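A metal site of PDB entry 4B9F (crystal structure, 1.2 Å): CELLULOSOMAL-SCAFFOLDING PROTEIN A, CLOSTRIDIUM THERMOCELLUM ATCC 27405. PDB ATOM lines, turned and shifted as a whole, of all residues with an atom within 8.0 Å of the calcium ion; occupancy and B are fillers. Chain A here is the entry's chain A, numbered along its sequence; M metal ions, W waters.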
ATOM      1  N   ASP A  13      -5.154  23.988  26.865  1.00  0.00           N
ATOM      2  CA  ASP A  13      -6.176  23.432  25.983  1.00  0.00           C
ATOM      3  C   ASP A  13      -7.520  24.142  26.172  1.00  0.00           C
ATOM      4  O   ASP A  13      -8.173  24.526  25.196  1.00  0.00           O
ATOM      5  CB  ASP A  13      -6.330  21.936  26.205  1.00  0.00           C
ATOM      6  CG  ASP A  13      -7.261  21.295  25.196  1.00  0.00           C
ATOM      7  OD1 ASP A  13      -7.215  21.695  24.020  1.00  0.00           O
ATOM      8  OD2 ASP A  13      -8.042  20.412  25.580  1.00  0.00           O
ATOM      9  N   ILE A  18      -7.949  33.425  23.229  1.00  0.00           N
ATOM     10  CA  ILE A  18      -6.989  32.909  22.255  1.00  0.00           C
ATOM     11  C   ILE A  18      -6.063  34.059  21.864  1.00  0.00           C
ATOM     12  O   ILE A  18      -6.522  35.188  21.668  1.00  0.00           O
ATOM     13  CB  ILE A  18      -7.706  32.280  21.044  1.00  0.00           C
ATOM     14  CG1 ILE A  18      -8.450  31.017  21.522  1.00  0.00           C
ATOM     15  CG2 ILE A  18      -6.702  31.897  19.947  1.00  0.00           C
ATOM     16  CD1 ILE A  18      -9.367  30.377  20.501  1.00  0.00           C
ATOM     17  N   TYR A  42      -7.195  30.128  11.809  1.00  0.00           N
ATOM     18  CA  TYR A  42      -8.332  29.230  11.687  1.00  0.00           C
ATOM     19  C   TYR A  42      -8.531  28.406  12.946  1.00  0.00           C
ATOM     20  O   TYR A  42      -7.571  27.868  13.514  1.00  0.00           O
ATOM     21  CB  TYR A  42      -8.125  28.278  10.520  1.00  0.00           C
ATOM     22  CG  TYR A  42      -7.801  28.916   9.198  1.00  0.00           C
ATOM     23  CD1 TYR A  42      -8.822  29.327   8.339  1.00  0.00           C
ATOM     24  CD2 TYR A  42      -6.488  29.039   8.762  1.00  0.00           C
ATOM     25  CE1 TYR A  42      -8.530  29.868   7.094  1.00  0.00           C
ATOM     26  CE2 TYR A  42      -6.178  29.596   7.521  1.00  0.00           C
ATOM     27  CZ  TYR A  42      -7.214  30.004   6.696  1.00  0.00           C
ATOM     28  OH  TYR A  42      -6.914  30.520   5.459  1.00  0.00           O
ATOM     29  N   TYR A  43      -9.784  28.238  13.349  1.00  0.00           N
ATOM     30  CA  TYR A  43     -10.078  27.510  14.572  1.00  0.00           C
ATOM     31  C   TYR A  43     -11.525  27.046  14.584  1.00  0.00           C
ATOM     32  O   TYR A  43     -12.297  27.338  13.670  1.00  0.00           O
ATOM     33  CB  TYR A  43      -9.789  28.408  15.791  1.00  0.00           C
ATOM     34  CG  TYR A  43     -10.679  29.628  15.918  1.00  0.00           C
ATOM     35  CD1 TYR A  43     -10.492  30.755  15.119  1.00  0.00           C
ATOM     36  CD2 TYR A  43     -11.724  29.652  16.833  1.00  0.00           C
ATOM     37  CE1 TYR A  43     -11.320  31.873  15.223  1.00  0.00           C
ATOM     38  CE2 TYR A  43     -12.560  30.757  16.952  1.00  0.00           C
ATOM     39  CZ  TYR A  43     -12.347  31.867  16.146  1.00  0.00           C
ATOM     40  OH  TYR A  43     -13.156  32.979  16.261  1.00  0.00           O
ATOM     41  N   THR A  44     -11.882  26.292  15.620  1.00  0.00           N
ATOM     42  CA  THR A  44     -13.267  25.900  15.846  1.00  0.00           C
ATOM     43  C   THR A  44     -13.790  26.675  17.046  1.00  0.00           C
ATOM     44  O   THR A  44     -13.178  26.673  18.118  1.00  0.00           O
ATOM     45  CB  THR A  44     -13.406  24.395  16.101  1.00  0.00           C
ATOM     46  OG1 THR A  44     -12.431  23.980  17.071  1.00  0.00           O
ATOM     47  CG2 THR A  44     -13.203  23.615  14.813  1.00  0.00           C
ATOM     48  N   VAL A  45     -14.929  27.329  16.877  1.00  0.00           N
ATOM     49  CA  VAL A  45     -15.449  28.236  17.894  1.00  0.00           C
ATOM     50  C   VAL A  45     -15.930  27.546  19.173  1.00  0.00           C
ATOM     51  O   VAL A  45     -15.952  28.153  20.229  1.00  0.00           O
ATOM     52  CB  VAL A  45     -16.545  29.164  17.279  1.00  0.00           C
ATOM     53  CG1 VAL A  45     -17.785  28.348  16.884  1.00  0.00           C
ATOM     54  CG2 VAL A  45     -16.903  30.311  18.213  1.00  0.00           C
ATOM     55  N   ASP A  46     -16.295  26.267  19.074  1.00  0.00           N
ATOM     56  CA  ASP A  46     -16.767  25.458  20.212  1.00  0.00           C
ATOM     57  C   ASP A  46     -17.983  26.084  20.895  1.00  0.00           C
ATOM     58  O   ASP A  46     -17.963  26.356  22.104  1.00  0.00           O
ATOM     59  CB  ASP A  46     -15.647  25.253  21.248  1.00  0.00           C
ATOM     60  CG  ASP A  46     -14.327  24.845  20.620  1.00  0.00           C
ATOM     61  OD1 ASP A  46     -14.304  23.954  19.733  1.00  0.00           O
ATOM     62  OD2 ASP A  46     -13.297  25.418  20.998  1.00  0.00           O
ATOM     63  N   GLY A  47     -19.048  26.287  20.120  1.00  0.00           N
ATOM     64  CA  GLY A  47     -20.246  26.939  20.613  1.00  0.00           C
ATOM     65  C   GLY A  47     -20.270  28.368  20.122  1.00  0.00           C
ATOM     66  O   GLY A  47     -19.559  29.223  20.632  1.00  0.00           O
ATOM     67  N   ASN A  86     -12.861  19.450  10.443  1.00  0.00           N
ATOM     68  CA  ASN A  86     -12.822  18.987  11.824  1.00  0.00           C
ATOM     69  C   ASN A  86     -12.117  19.950  12.764  1.00  0.00           C
ATOM     70  O   ASN A  86     -12.383  19.965  13.967  1.00  0.00           O
ATOM     71  CB  ASN A  86     -12.153  17.610  11.917  1.00  0.00           C
ATOM     72  CG  ASN A  86     -13.029  16.491  11.393  1.00  0.00           C
ATOM     73  OD1 ASN A  86     -14.247  16.625  11.321  1.00  0.00           O
ATOM     74  ND2 ASN A  86     -12.408  15.366  11.044  1.00  0.00           N
ATOM     75  N   ASN A  87     -11.221  20.763  12.203  1.00  0.00           N
ATOM     76  CA  ASN A  87     -10.428  21.675  13.005  1.00  0.00           C
ATOM     77  C   ASN A  87     -10.557  23.136  12.607  1.00  0.00           C
ATOM     78  O   ASN A  87      -9.812  23.985  13.084  1.00  0.00           O
ATOM     79  CB  ASN A  87      -8.956  21.252  12.995  1.00  0.00           C
ATOM     80  CG  ASN A  87      -8.733  19.882  13.609  1.00  0.00           C
ATOM     81  OD1 ASN A  87      -8.597  19.760  14.825  1.00  0.00           O
ATOM     82  ND2 ASN A  87      -8.692  18.859  12.776  1.00  0.00           N
ATOM     83  N   ALA A  88     -11.514  23.447  11.734  1.00  0.00           N
ATOM     84  CA  ALA A  88     -11.713  24.834  11.324  1.00  0.00           C
ATOM     85  C   ALA A  88     -13.152  25.096  10.930  1.00  0.00           C
ATOM     86  O   ALA A  88     -13.639  24.516   9.949  1.00  0.00           O
ATOM     87  CB  ALA A  88     -10.759  25.213  10.175  1.00  0.00           C
ATOM     88  N   ASP A  89     -13.823  25.965  11.666  1.00  0.00           N
ATOM     89  CA  ASP A  89     -15.133  26.456  11.238  1.00  0.00           C
ATOM     90  C   ASP A  89     -15.209  27.967  11.168  1.00  0.00           C
ATOM     91  O   ASP A  89     -16.207  28.513  10.695  1.00  0.00           O
ATOM     92  CB  ASP A  89     -16.302  25.887  12.088  1.00  0.00           C
ATOM     93  CG  ASP A  89     -16.167  26.170  13.580  1.00  0.00           C
ATOM     94  OD1 ASP A  89     -15.716  27.251  14.003  1.00  0.00           O
ATOM     95  OD2 ASP A  89     -16.561  25.274  14.349  1.00  0.00           O
ATOM     96  N   LYS A 115     -14.893  35.251  23.525  1.00  0.00           N
ATOM     97  CA  LYS A 115     -16.342  35.317  23.389  1.00  0.00           C
ATOM     98  C   LYS A 115     -16.868  36.397  24.317  1.00  0.00           C
ATOM     99  O   LYS A 115     -16.294  36.651  25.380  1.00  0.00           O
ATOM    100  CB  LYS A 115     -16.958  33.972  23.735  1.00  0.00           C
ATOM    101  CG  LYS A 115     -16.576  32.887  22.747  1.00  0.00           C
ATOM    102  CD  LYS A 115     -17.007  31.534  23.240  1.00  0.00           C
ATOM    103  CE  LYS A 115     -16.726  30.485  22.205  1.00  0.00           C
ATOM    104  NZ  LYS A 115     -17.127  29.113  22.628  1.00  0.00           N
ATOM    105  N   ASN A 120     -15.633  29.233  27.419  1.00  0.00           N
ATOM    106  CA  ASN A 120     -14.392  28.575  27.031  1.00  0.00           C
ATOM    107  C   ASN A 120     -14.282  28.141  25.580  1.00  0.00           C
ATOM    108  O   ASN A 120     -15.272  27.843  24.916  1.00  0.00           O
ATOM    109  CB  ASN A 120     -14.134  27.369  27.936  1.00  0.00           C
ATOM    110  CG  ASN A 120     -13.720  27.766  29.334  1.00  0.00           C
ATOM    111  OD1 ASN A 120     -13.182  28.852  29.548  1.00  0.00           O
ATOM    112  ND2 ASN A 120     -13.956  26.884  30.298  1.00  0.00           N
ATOM    113  N   TYR A 121     -13.037  28.146  25.116  1.00  0.00           N
ATOM    114  CA  TYR A 121     -12.616  27.496  23.882  1.00  0.00           C
ATOM    115  C   TYR A 121     -11.785  26.262  24.230  1.00  0.00           C
ATOM    116  O   TYR A 121     -11.215  26.157  25.320  1.00  0.00           O
ATOM    117  CB  TYR A 121     -11.679  28.398  23.108  1.00  0.00           C
ATOM    118  CG  TYR A 121     -12.204  29.694  22.565  1.00  0.00           C
ATOM    119  CD1 TYR A 121     -12.971  29.728  21.389  1.00  0.00           C
ATOM    120  CD2 TYR A 121     -11.888  30.897  23.181  1.00  0.00           C
ATOM    121  CE1 TYR A 121     -13.417  30.937  20.858  1.00  0.00           C
ATOM    122  CE2 TYR A 121     -12.337  32.105  22.672  1.00  0.00           C
ATOM    123  CZ  TYR A 121     -13.090  32.124  21.510  1.00  0.00           C
ATOM    124  OH  TYR A 121     -13.507  33.327  21.000  1.00  0.00           O
ATOM    125  N   THR A 122     -11.688  25.370  23.253  1.00  0.00           N
ATOM    126  CA  THR A 122     -10.779  24.236  23.286  1.00  0.00           C
ATOM    127  C   THR A 122      -9.785  24.431  22.153  1.00  0.00           C
ATOM    128  O   THR A 122     -10.197  24.594  20.999  1.00  0.00           O
ATOM    129  CB  THR A 122     -11.555  22.940  23.036  1.00  0.00           C
ATOM    130  OG1 THR A 122     -12.446  22.700  24.133  1.00  0.00           O
ATOM    131  CG2 THR A 122     -10.609  21.755  22.861  1.00  0.00           C
ATOM    132  N   GLN A 123      -8.484  24.436  22.457  1.00  0.00           N
ATOM    133  CA  GLN A 123      -7.498  24.742  21.414  1.00  0.00           C
ATOM    134  C   GLN A 123      -7.010  23.523  20.632  1.00  0.00           C
ATOM    135  O   GLN A 123      -6.433  23.681  19.568  1.00  0.00           O
ATOM    136  CB  GLN A 123      -6.331  25.534  21.993  1.00  0.00           C
ATOM    137  CG  GLN A 123      -6.761  26.809  22.688  1.00  0.00           C
ATOM    138  CD  GLN A 123      -5.641  27.825  22.782  1.00  0.00           C
ATOM    139  OE1 GLN A 123      -5.439  28.625  21.870  1.00  0.00           O
ATOM    140  NE2 GLN A 123      -4.902  27.787  23.877  1.00  0.00           N
ATOM    141  N   SER A 124      -7.255  22.325  21.163  1.00  0.00           N
ATOM    142  CA  SER A 124      -6.727  21.104  20.558  1.00  0.00           C
ATOM    143  C   SER A 124      -7.390  20.783  19.228  1.00  0.00           C
ATOM    144  O   SER A 124      -6.893  19.945  18.486  1.00  0.00           O
ATOM    145  CB  SER A 124      -6.887  19.925  21.510  1.00  0.00           C
ATOM    146  OG  SER A 124      -8.268  19.619  21.685  1.00  0.00           O
ATOM    147  N   ASN A 125      -8.524  21.402  18.943  1.00  0.00           N
ATOM    148  CA  ASN A 125      -9.241  21.187  17.688  1.00  0.00           C
ATOM    149  C   ASN A 125      -9.245  22.432  16.802  1.00  0.00           C
ATOM    150  O   ASN A 125     -10.198  22.688  16.074  1.00  0.00           O
ATOM    151  CB  ASN A 125     -10.668  20.671  17.938  1.00  0.00           C
ATOM    152  CG  ASN A 125     -11.491  21.635  18.771  1.00  0.00           C
ATOM    153  OD1 ASN A 125     -11.012  22.698  19.156  1.00  0.00           O
ATOM    154  ND2 ASN A 125     -12.757  21.282  19.016  1.00  0.00           N
ATOM    155  N   ASP A 126      -8.155  23.207  16.884  1.00  0.00           N
ATOM    156  CA  ASP A 126      -7.986  24.432  16.096  1.00  0.00           C
ATOM    157  C   ASP A 126      -6.829  24.284  15.108  1.00  0.00           C
ATOM    158  O   ASP A 126      -5.677  24.145  15.515  1.00  0.00           O
ATOM    159  CB  ASP A 126      -7.686  25.634  16.999  1.00  0.00           C
ATOM    160  CG  ASP A 126      -8.827  25.962  17.946  1.00  0.00           C
ATOM    161  OD1 ASP A 126      -9.948  25.480  17.715  1.00  0.00           O
ATOM    162  OD2 ASP A 126      -8.592  26.729  18.906  1.00  0.00           O
ATOM    163  N   TYR A 127      -7.146  24.346  13.822  1.00  0.00           N
ATOM    164  CA  TYR A 127      -6.158  24.137  12.752  1.00  0.00           C
ATOM    165  C   TYR A 127      -4.890  24.990  12.910  1.00  0.00           C
ATOM    166  O   TYR A 127      -3.781  24.488  12.744  1.00  0.00           O
ATOM    167  CB  TYR A 127      -6.827  24.429  11.417  1.00  0.00           C
ATOM    168  CG  TYR A 127      -5.984  24.346  10.158  1.00  0.00           C
ATOM    169  CD1 TYR A 127      -5.717  23.121   9.554  1.00  0.00           C
ATOM    170  CD2 TYR A 127      -5.519  25.496   9.530  1.00  0.00           C
ATOM    171  CE1 TYR A 127      -4.998  23.051   8.375  1.00  0.00           C
ATOM    172  CE2 TYR A 127      -4.787  25.427   8.339  1.00  0.00           C
ATOM    173  CZ  TYR A 127      -4.526  24.199   7.779  1.00  0.00           C
ATOM    174  OH  TYR A 127      -3.835  24.114   6.586  1.00  0.00           O
HETATM  175 CA    CA M   1     -11.760  24.997  19.234  1.00  0.00          CA
HETATM  176  O   HOH W   1     -10.970  27.237  20.000  1.00  0.00           O
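O of Asp 46 lies within hydrogen-bond range of NZ of Lys 115 (2.9 Å).
The calcium ion is bound by the side-chain carboxylate (OD2) of Asp 46, the backbone carbonyl oxygen (O) of Thr 122, the side-chain carboxylate (OD1) of Asp 126, the side-chain amide oxygen (OD1) of Asn 125, the backbone carbonyl oxygen (O) of Thr 44, the side-chain hydroxyl (OG1) of Thr 44, water W1 and the side-chain carboxylate (OD1) of Asp 46.
The calcium ion has eight donor atoms within binding distance.
Five residues have an atom within 4 Å of the calcium ion: Thr 44, Asp 46, Thr 122, Asn 125 and Asp 126.
Along chain A the residues within 4 Å of the calcium ion span positions 44 to 126.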
